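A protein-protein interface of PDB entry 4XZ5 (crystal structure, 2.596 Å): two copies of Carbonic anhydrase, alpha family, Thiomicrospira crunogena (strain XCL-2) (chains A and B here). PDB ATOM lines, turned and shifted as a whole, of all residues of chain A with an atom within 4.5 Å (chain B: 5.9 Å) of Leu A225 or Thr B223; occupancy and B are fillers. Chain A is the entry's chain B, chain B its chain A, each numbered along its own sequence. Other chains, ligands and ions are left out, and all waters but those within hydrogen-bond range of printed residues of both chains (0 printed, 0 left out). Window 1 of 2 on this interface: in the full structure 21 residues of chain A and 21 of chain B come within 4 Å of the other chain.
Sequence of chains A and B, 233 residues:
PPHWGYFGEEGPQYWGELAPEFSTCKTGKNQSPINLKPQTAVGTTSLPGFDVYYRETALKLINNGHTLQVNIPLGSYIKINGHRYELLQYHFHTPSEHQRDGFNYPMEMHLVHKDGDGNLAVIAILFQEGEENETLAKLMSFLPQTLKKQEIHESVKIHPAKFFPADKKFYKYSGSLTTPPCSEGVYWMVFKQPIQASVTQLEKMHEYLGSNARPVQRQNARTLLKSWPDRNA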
ATOM      1  N   VAL A  42     -23.200  -8.553  20.219  1.00  0.00           N
ATOM      2  CA  VAL A  42     -23.059  -9.262  18.958  1.00  0.00           C
ATOM      3  C   VAL A  42     -22.793 -10.763  19.177  1.00  0.00           C
ATOM      4  O   VAL A  42     -21.833 -11.156  19.836  1.00  0.00           O
ATOM      5  CB  VAL A  42     -21.920  -8.603  18.143  1.00  0.00           C
ATOM      6  CG1 VAL A  42     -21.586  -9.383  16.855  1.00  0.00           C
ATOM      7  CG2 VAL A  42     -22.296  -7.161  17.845  1.00  0.00           C
ATOM      8  N   THR A  44     -21.737 -14.650  18.414  1.00  0.00           N
ATOM      9  CA  THR A  44     -20.516 -15.168  17.806  1.00  0.00           C
ATOM     10  C   THR A  44     -20.610 -16.649  17.424  1.00  0.00           C
ATOM     11  O   THR A  44     -21.470 -17.390  17.904  1.00  0.00           O
ATOM     12  CB  THR A  44     -19.296 -14.961  18.738  1.00  0.00           C
ATOM     13  OG1 THR A  44     -19.493 -15.677  19.969  1.00  0.00           O
ATOM     14  CG2 THR A  44     -19.084 -13.465  19.019  1.00  0.00           C
ATOM     15  N   LEU A  47     -16.038 -17.756  19.262  1.00  0.00           N
ATOM     16  CA  LEU A  47     -15.355 -17.153  20.393  1.00  0.00           C
ATOM     17  C   LEU A  47     -14.829 -18.279  21.252  1.00  0.00           C
ATOM     18  O   LEU A  47     -15.522 -19.260  21.482  1.00  0.00           O
ATOM     19  CB  LEU A  47     -16.293 -16.241  21.195  1.00  0.00           C
ATOM     20  CG  LEU A  47     -15.765 -15.383  22.357  1.00  0.00           C
ATOM     21  CD1 LEU A  47     -14.823 -14.248  21.925  1.00  0.00           C
ATOM     22  CD2 LEU A  47     -16.935 -14.791  23.134  1.00  0.00           C
ATOM     23  N   PHE A 170     -21.852 -16.234  28.352  1.00  0.00           N
ATOM     24  CA  PHE A 170     -21.210 -15.032  28.872  1.00  0.00           C
ATOM     25  C   PHE A 170     -21.028 -13.935  27.831  1.00  0.00           C
ATOM     26  O   PHE A 170     -21.092 -14.175  26.625  1.00  0.00           O
ATOM     27  CB  PHE A 170     -19.849 -15.374  29.510  1.00  0.00           C
ATOM     28  CG  PHE A 170     -18.849 -15.967  28.557  1.00  0.00           C
ATOM     29  CD1 PHE A 170     -17.926 -15.158  27.895  1.00  0.00           C
ATOM     30  CD2 PHE A 170     -18.787 -17.347  28.362  1.00  0.00           C
ATOM     31  CE1 PHE A 170     -16.985 -15.711  27.026  1.00  0.00           C
ATOM     32  CE2 PHE A 170     -17.841 -17.917  27.500  1.00  0.00           C
ATOM     33  CZ  PHE A 170     -16.955 -17.099  26.820  1.00  0.00           C
ATOM     34  N   TYR A 171     -20.812 -12.723  28.338  1.00  0.00           N
ATOM     35  CA  TYR A 171     -20.455 -11.565  27.538  1.00  0.00           C
ATOM     36  C   TYR A 171     -18.956 -11.379  27.664  1.00  0.00           C
ATOM     37  O   TYR A 171     -18.401 -11.591  28.744  1.00  0.00           O
ATOM     38  CB  TYR A 171     -21.191 -10.324  28.028  1.00  0.00           C
ATOM     39  CG  TYR A 171     -22.702 -10.448  27.938  1.00  0.00           C
ATOM     40  CD1 TYR A 171     -23.339 -10.523  26.710  1.00  0.00           C
ATOM     41  CD2 TYR A 171     -23.499 -10.462  29.085  1.00  0.00           C
ATOM     42  CE1 TYR A 171     -24.717 -10.621  26.616  1.00  0.00           C
ATOM     43  CE2 TYR A 171     -24.891 -10.561  28.998  1.00  0.00           C
ATOM     44  CZ  TYR A 171     -25.487 -10.637  27.756  1.00  0.00           C
ATOM     45  OH  TYR A 171     -26.858 -10.735  27.635  1.00  0.00           O
ATOM     46  N   LYS A 172     -18.283 -11.018  26.575  1.00  0.00           N
ATOM     47  CA  LYS A 172     -16.849 -10.743  26.668  1.00  0.00           C
ATOM     48  C   LYS A 172     -16.481  -9.428  25.982  1.00  0.00           C
ATOM     49  O   LYS A 172     -17.020  -9.065  24.934  1.00  0.00           O
ATOM     50  CB  LYS A 172     -16.042 -11.940  26.113  1.00  0.00           C
ATOM     51  CG  LYS A 172     -15.085 -11.665  24.975  1.00  0.00           C
ATOM     52  CD  LYS A 172     -13.681 -11.319  25.420  1.00  0.00           C
ATOM     53  CE  LYS A 172     -13.037 -10.414  24.363  1.00  0.00           C
ATOM     54  NZ  LYS A 172     -11.666  -9.921  24.641  1.00  0.00           N
ATOM     55  N   THR A 223     -16.812  -3.393  20.878  1.00  0.00           N
ATOM     56  CA  THR A 223     -17.986  -4.216  20.612  1.00  0.00           C
ATOM     57  C   THR A 223     -18.193  -5.194  21.777  1.00  0.00           C
ATOM     58  O   THR A 223     -17.253  -5.836  22.230  1.00  0.00           O
ATOM     59  CB  THR A 223     -17.830  -4.986  19.296  1.00  0.00           C
ATOM     60  OG1 THR A 223     -17.782  -4.053  18.207  1.00  0.00           O
ATOM     61  CG2 THR A 223     -18.985  -5.950  19.106  1.00  0.00           C
ATOM     62  N   LEU A 224     -19.406  -5.288  22.295  1.00  0.00           N
ATOM     63  CA  LEU A 224     -19.688  -6.261  23.343  1.00  0.00           C
ATOM     64  C   LEU A 224     -20.051  -7.618  22.699  1.00  0.00           C
ATOM     65  O   LEU A 224     -20.989  -7.692  21.909  1.00  0.00           O
ATOM     66  CB  LEU A 224     -20.818  -5.750  24.270  1.00  0.00           C
ATOM     67  CG  LEU A 224     -21.212  -6.665  25.457  1.00  0.00           C
ATOM     68  CD1 LEU A 224     -20.064  -6.836  26.449  1.00  0.00           C
ATOM     69  CD2 LEU A 224     -22.479  -6.191  26.188  1.00  0.00           C
ATOM     70  N   LEU A 225     -19.314  -8.685  23.021  1.00  0.00           N
ATOM     71  CA  LEU A 225     -19.555  -9.999  22.386  1.00  0.00           C
ATOM     72  C   LEU A 225     -20.390 -10.949  23.258  1.00  0.00           C
ATOM     73  O   LEU A 225     -20.279 -10.939  24.488  1.00  0.00           O
ATOM     74  CB  LEU A 225     -18.226 -10.676  22.043  1.00  0.00           C
ATOM     75  CG  LEU A 225     -17.284  -9.754  21.271  1.00  0.00           C
ATOM     76  CD1 LEU A 225     -15.942 -10.410  20.998  1.00  0.00           C
ATOM     77  CD2 LEU A 225     -17.949  -9.317  19.981  1.00  0.00           C
ATOM     78  N   LYS A 226     -21.240 -11.754  22.626  1.00  0.00           N
ATOM     79  CA  LYS A 226     -21.892 -12.866  23.327  1.00  0.00           C
ATOM     80  C   LYS A 226     -21.139 -14.141  22.972  1.00  0.00           C
ATOM     81  O   LYS A 226     -20.650 -14.272  21.846  1.00  0.00           O
ATOM     82  CB  LYS A 226     -23.363 -13.011  22.938  1.00  0.00           C
ATOM     83  CG  LYS A 226     -24.086 -11.730  22.653  1.00  0.00           C
ATOM     84  CD  LYS A 226     -25.577 -11.936  22.691  1.00  0.00           C
ATOM     85  CE  LYS A 226     -26.147 -11.998  21.286  1.00  0.00           C
ATOM     86  NZ  LYS A 226     -27.535 -11.466  21.229  1.00  0.00           N
ATOM     87  N   SER A 227     -21.093 -15.097  23.898  1.00  0.00           N
ATOM     88  CA  SER A 227     -20.351 -16.345  23.675  1.00  0.00           C
ATOM     89  C   SER A 227     -21.125 -17.360  22.840  1.00  0.00           C
ATOM     90  O   SER A 227     -20.611 -18.440  22.570  1.00  0.00           O
ATOM     91  CB  SER A 227     -19.953 -16.981  25.019  1.00  0.00           C
ATOM     92  OG  SER A 227     -21.083 -17.394  25.778  1.00  0.00           O
ATOM     93  N   VAL B  42     -12.717 -14.156  14.995  1.00  0.00           N
ATOM     94  CA  VAL B  42     -13.992 -14.685  15.474  1.00  0.00           C
ATOM     95  C   VAL B  42     -15.193 -14.279  14.616  1.00  0.00           C
ATOM     96  O   VAL B  42     -15.486 -13.087  14.435  1.00  0.00           O
ATOM     97  CB  VAL B  42     -14.239 -14.240  16.937  1.00  0.00           C
ATOM     98  CG1 VAL B  42     -15.649 -14.584  17.397  1.00  0.00           C
ATOM     99  CG2 VAL B  42     -13.182 -14.833  17.838  1.00  0.00           C
ATOM    100  N   THR B  44     -19.092 -13.672  13.493  1.00  0.00           N
ATOM    101  CA  THR B  44     -20.194 -13.019  14.164  1.00  0.00           C
ATOM    102  C   THR B  44     -21.479 -13.277  13.408  1.00  0.00           C
ATOM    103  O   THR B  44     -21.461 -13.708  12.241  1.00  0.00           O
ATOM    104  CB  THR B  44     -19.964 -11.506  14.309  1.00  0.00           C
ATOM    105  OG1 THR B  44     -19.766 -10.933  13.011  1.00  0.00           O
ATOM    106  CG2 THR B  44     -18.733 -11.218  15.161  1.00  0.00           C
ATOM    107  N   LYS B 172     -13.168  -6.289  12.206  1.00  0.00           N
ATOM    108  CA  LYS B 172     -13.320  -5.105  13.050  1.00  0.00           C
ATOM    109  C   LYS B 172     -12.658  -5.329  14.412  1.00  0.00           C
ATOM    110  O   LYS B 172     -12.681  -6.434  14.948  1.00  0.00           O
ATOM    111  CB  LYS B 172     -14.814  -4.708  13.168  1.00  0.00           C
ATOM    112  CG  LYS B 172     -15.367  -4.493  14.587  1.00  0.00           C
ATOM    113  CD  LYS B 172     -15.026  -3.173  15.241  1.00  0.00           C
ATOM    114  CE  LYS B 172     -15.088  -3.349  16.748  1.00  0.00           C
ATOM    115  NZ  LYS B 172     -15.367  -2.111  17.501  1.00  0.00           N
ATOM    116  N   TYR B 173     -12.042  -4.278  14.948  1.00  0.00           N
ATOM    117  CA  TYR B 173     -11.456  -4.317  16.291  1.00  0.00           C
ATOM    118  C   TYR B 173     -11.324  -2.906  16.844  1.00  0.00           C
ATOM    119  O   TYR B 173     -11.377  -1.931  16.107  1.00  0.00           O
ATOM    120  CB  TYR B 173     -10.078  -5.011  16.303  1.00  0.00           C
ATOM    121  CG  TYR B 173      -8.932  -4.196  15.699  1.00  0.00           C
ATOM    122  CD1 TYR B 173      -8.688  -4.194  14.321  1.00  0.00           C
ATOM    123  CD2 TYR B 173      -8.097  -3.434  16.495  1.00  0.00           C
ATOM    124  CE1 TYR B 173      -7.646  -3.460  13.763  1.00  0.00           C
ATOM    125  CE2 TYR B 173      -7.051  -2.687  15.931  1.00  0.00           C
ATOM    126  CZ  TYR B 173      -6.838  -2.710  14.576  1.00  0.00           C
ATOM    127  OH  TYR B 173      -5.804  -1.991  14.033  1.00  0.00           O
ATOM    128  N   SER B 174     -11.134  -2.815  18.150  1.00  0.00           N
ATOM    129  CA  SER B 174     -10.984  -1.543  18.812  1.00  0.00           C
ATOM    130  C   SER B 174      -9.511  -1.186  18.862  1.00  0.00           C
ATOM    131  O   SER B 174      -8.714  -1.926  19.420  1.00  0.00           O
ATOM    132  CB  SER B 174     -11.594  -1.596  20.220  1.00  0.00           C
ATOM    133  OG  SER B 174     -11.274  -0.432  20.957  1.00  0.00           O
ATOM    134  N   GLN B 219      -1.792  -7.490  20.272  1.00  0.00           N
ATOM    135  CA  GLN B 219      -3.234  -7.607  20.322  1.00  0.00           C
ATOM    136  C   GLN B 219      -3.766  -7.563  21.761  1.00  0.00           C
ATOM    137  O   GLN B 219      -4.856  -7.034  21.999  1.00  0.00           O
ATOM    138  CB  GLN B 219      -3.684  -8.885  19.603  1.00  0.00           C
ATOM    139  CG  GLN B 219      -5.195  -9.051  19.490  1.00  0.00           C
ATOM    140  CD  GLN B 219      -5.615  -9.906  18.307  1.00  0.00           C
ATOM    141  OE1 GLN B 219      -5.004  -9.835  17.237  1.00  0.00           O
ATOM    142  NE2 GLN B 219      -6.642 -10.738  18.498  1.00  0.00           N
ATOM    143  N   ALA B 221      -5.631  -8.075  25.054  1.00  0.00           N
ATOM    144  CA  ALA B 221      -6.910  -8.690  25.415  1.00  0.00           C
ATOM    145  C   ALA B 221      -7.975  -8.614  24.303  1.00  0.00           C
ATOM    146  O   ALA B 221      -9.116  -9.029  24.508  1.00  0.00           O
ATOM    147  CB  ALA B 221      -7.454  -8.051  26.704  1.00  0.00           C
ATOM    148  N   ARG B 222      -7.611  -8.107  23.128  1.00  0.00           N
ATOM    149  CA  ARG B 222      -8.626  -7.852  22.108  1.00  0.00           C
ATOM    150  C   ARG B 222      -8.997  -9.068  21.294  1.00  0.00           C
ATOM    151  O   ARG B 222      -8.166  -9.922  21.008  1.00  0.00           O
ATOM    152  CB  ARG B 222      -8.165  -6.737  21.173  1.00  0.00           C
ATOM    153  CG  ARG B 222      -8.095  -5.380  21.855  1.00  0.00           C
ATOM    154  CD  ARG B 222      -7.424  -4.362  20.959  1.00  0.00           C
ATOM    155  NE  ARG B 222      -5.999  -4.630  20.793  1.00  0.00           N
ATOM    156  CZ  ARG B 222      -5.200  -3.868  20.059  1.00  0.00           C
ATOM    157  NH1 ARG B 222      -5.712  -2.816  19.438  1.00  0.00           N
ATOM    158  NH2 ARG B 222      -3.912  -4.161  19.930  1.00  0.00           N
ATOM    159  N   THR B 223     -10.267  -9.116  20.913  1.00  0.00           N
ATOM    160  CA  THR B 223     -10.753 -10.115  19.973  1.00  0.00           C
ATOM    161  C   THR B 223     -10.851  -9.496  18.575  1.00  0.00           C
ATOM    162  O   THR B 223     -11.381  -8.397  18.407  1.00  0.00           O
ATOM    163  CB  THR B 223     -12.129 -10.650  20.377  1.00  0.00           C
ATOM    164  OG1 THR B 223     -12.024 -11.309  21.639  1.00  0.00           O
ATOM    165  CG2 THR B 223     -12.651 -11.636  19.331  1.00  0.00           C
ATOM    166  N   LEU B 224     -10.304 -10.187  17.583  1.00  0.00           N
ATOM    167  CA  LEU B 224     -10.453  -9.763  16.197  1.00  0.00           C
ATOM    168  C   LEU B 224     -11.750 -10.361  15.627  1.00  0.00           C
ATOM    169  O   LEU B 224     -11.945 -11.593  15.640  1.00  0.00           O
ATOM    170  CB  LEU B 224      -9.228 -10.183  15.364  1.00  0.00           C
ATOM    171  CG  LEU B 224      -9.214  -9.762  13.900  1.00  0.00           C
ATOM    172  CD1 LEU B 224      -9.168  -8.234  13.799  1.00  0.00           C
ATOM    173  CD2 LEU B 224      -8.037 -10.390  13.179  1.00  0.00           C
ATOM    174  N   LEU B 225     -12.649  -9.500  15.157  1.00  0.00           N
ATOM    175  CA  LEU B 225     -13.939  -9.973  14.647  1.00  0.00           C
ATOM    176  C   LEU B 225     -13.959 -10.040  13.131  1.00  0.00           C
ATOM    177  O   LEU B 225     -13.308  -9.246  12.468  1.00  0.00           O
ATOM    178  CB  LEU B 225     -15.078  -9.082  15.137  1.00  0.00           C
ATOM    179  CG  LEU B 225     -15.130  -8.854  16.646  1.00  0.00           C
ATOM    180  CD1 LEU B 225     -16.235  -7.873  17.000  1.00  0.00           C
ATOM    181  CD2 LEU B 225     -15.343 -10.183  17.368  1.00  0.00           C
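OG1 of Thr A223 lies close to NZ of Lys B172.
NZ of Lys A172 sits at hydrogen-bond distance from O of Ala B221 (2.7 Å).
The side-chain amino group (NZ) of Lys A172 lies close to the side-chain hydroxyl (OG1) of Thr B223 (3.3 Å).
The backbone NH of Val B42 lies within hydrogen-bond range of the backbone carbonyl oxygen of Leu B224, 2.8 Å away.
N of Lys B172 is in hydrogen-bond range of O of Leu B225, 3.0 Å away.
The backbone NH (N) of Val A42 lies within hydrogen-bond range of the backbone carbonyl oxygen (O) of Leu A224, 2.9 Å away.
The backbone carbonyl oxygen of Val A42 lies within hydrogen-bond range of the backbone NH of Lys A226, 2.9 Å away.
The side-chain hydroxyl (OG1) of Thr A44 sits at hydrogen-bond distance from the backbone carbonyl oxygen (O) of Lys A226 (2.6 Å).
The backbone NH of Lys A172 is in hydrogen-bond range of the backbone carbonyl oxygen of Leu A225.
CG1 of Val A42 touches CB of Thr B44, 3.7 Å away.
CG1 of Val B42 touches CB of Thr A44, at 3.9 Å.
Leu A47 touches Val B42.
Leu B225 touches Thr A223 (CD1 to CG2, 3.96 Å).
Leu A225 touches Thr B223 (CD1 to CB, 3.9 Å).
Leu B225 touches Leu A225 (CD2 to CD1, 3.7 Å).
Leu A225 touches two residues of chain B.
Thr B223 touches just these residues of chain A: Lys A172 and Leu A225.
Printed residues of chain B within 4 Å of Lys A172: Ala B221 and Thr B223.
Printed residues of chain A within 4 Å of Val B42: Thr A44 and Leu A47.
Of the printed residues of chain B, Thr A223 touches Lys B172 (3.1 Å) and Leu B225 (3.96 Å).
Printed residues of chain B within 4 Å of Val A42: Thr B44 (3.7 Å).
Printed residues of chain A within 4 Å of Ala B221: Lys A172 (2.7 Å).
The nearest residue of chain B that does not touch Leu A225 is Thr B44 (5.2 Å).
Hydrophobic or aromatic side chains of chain B within 4 Å of the printed part of chain A: Val B42 and Leu B225.
Of the 11 printed residues of chain A, 6 touch a printed residue of chain B.
Hydrophobic or aromatic side chains of chain A within 4 Å of the printed part of chain B: Val A42 and Leu A225.
Among the printed residues, 9 pairs touch across the chains.
Among the printed residues, no Asp or Glu carboxylate lies within 4 Å of a Lys or Arg side-chain nitrogen of the other chain.
Val A42 touches Thr B44, and with the chains exchanged Thr A44 touches Val B42.
Lys A172 touches Thr B223, and with the chains exchanged Thr A223 touches Lys B172.
Thr A223 touches Leu B225, and with the chains exchanged Leu A225 touches Thr B223.
Leu B225 touches its own counterpart, Leu A225.
6 positions are printed for both chains.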
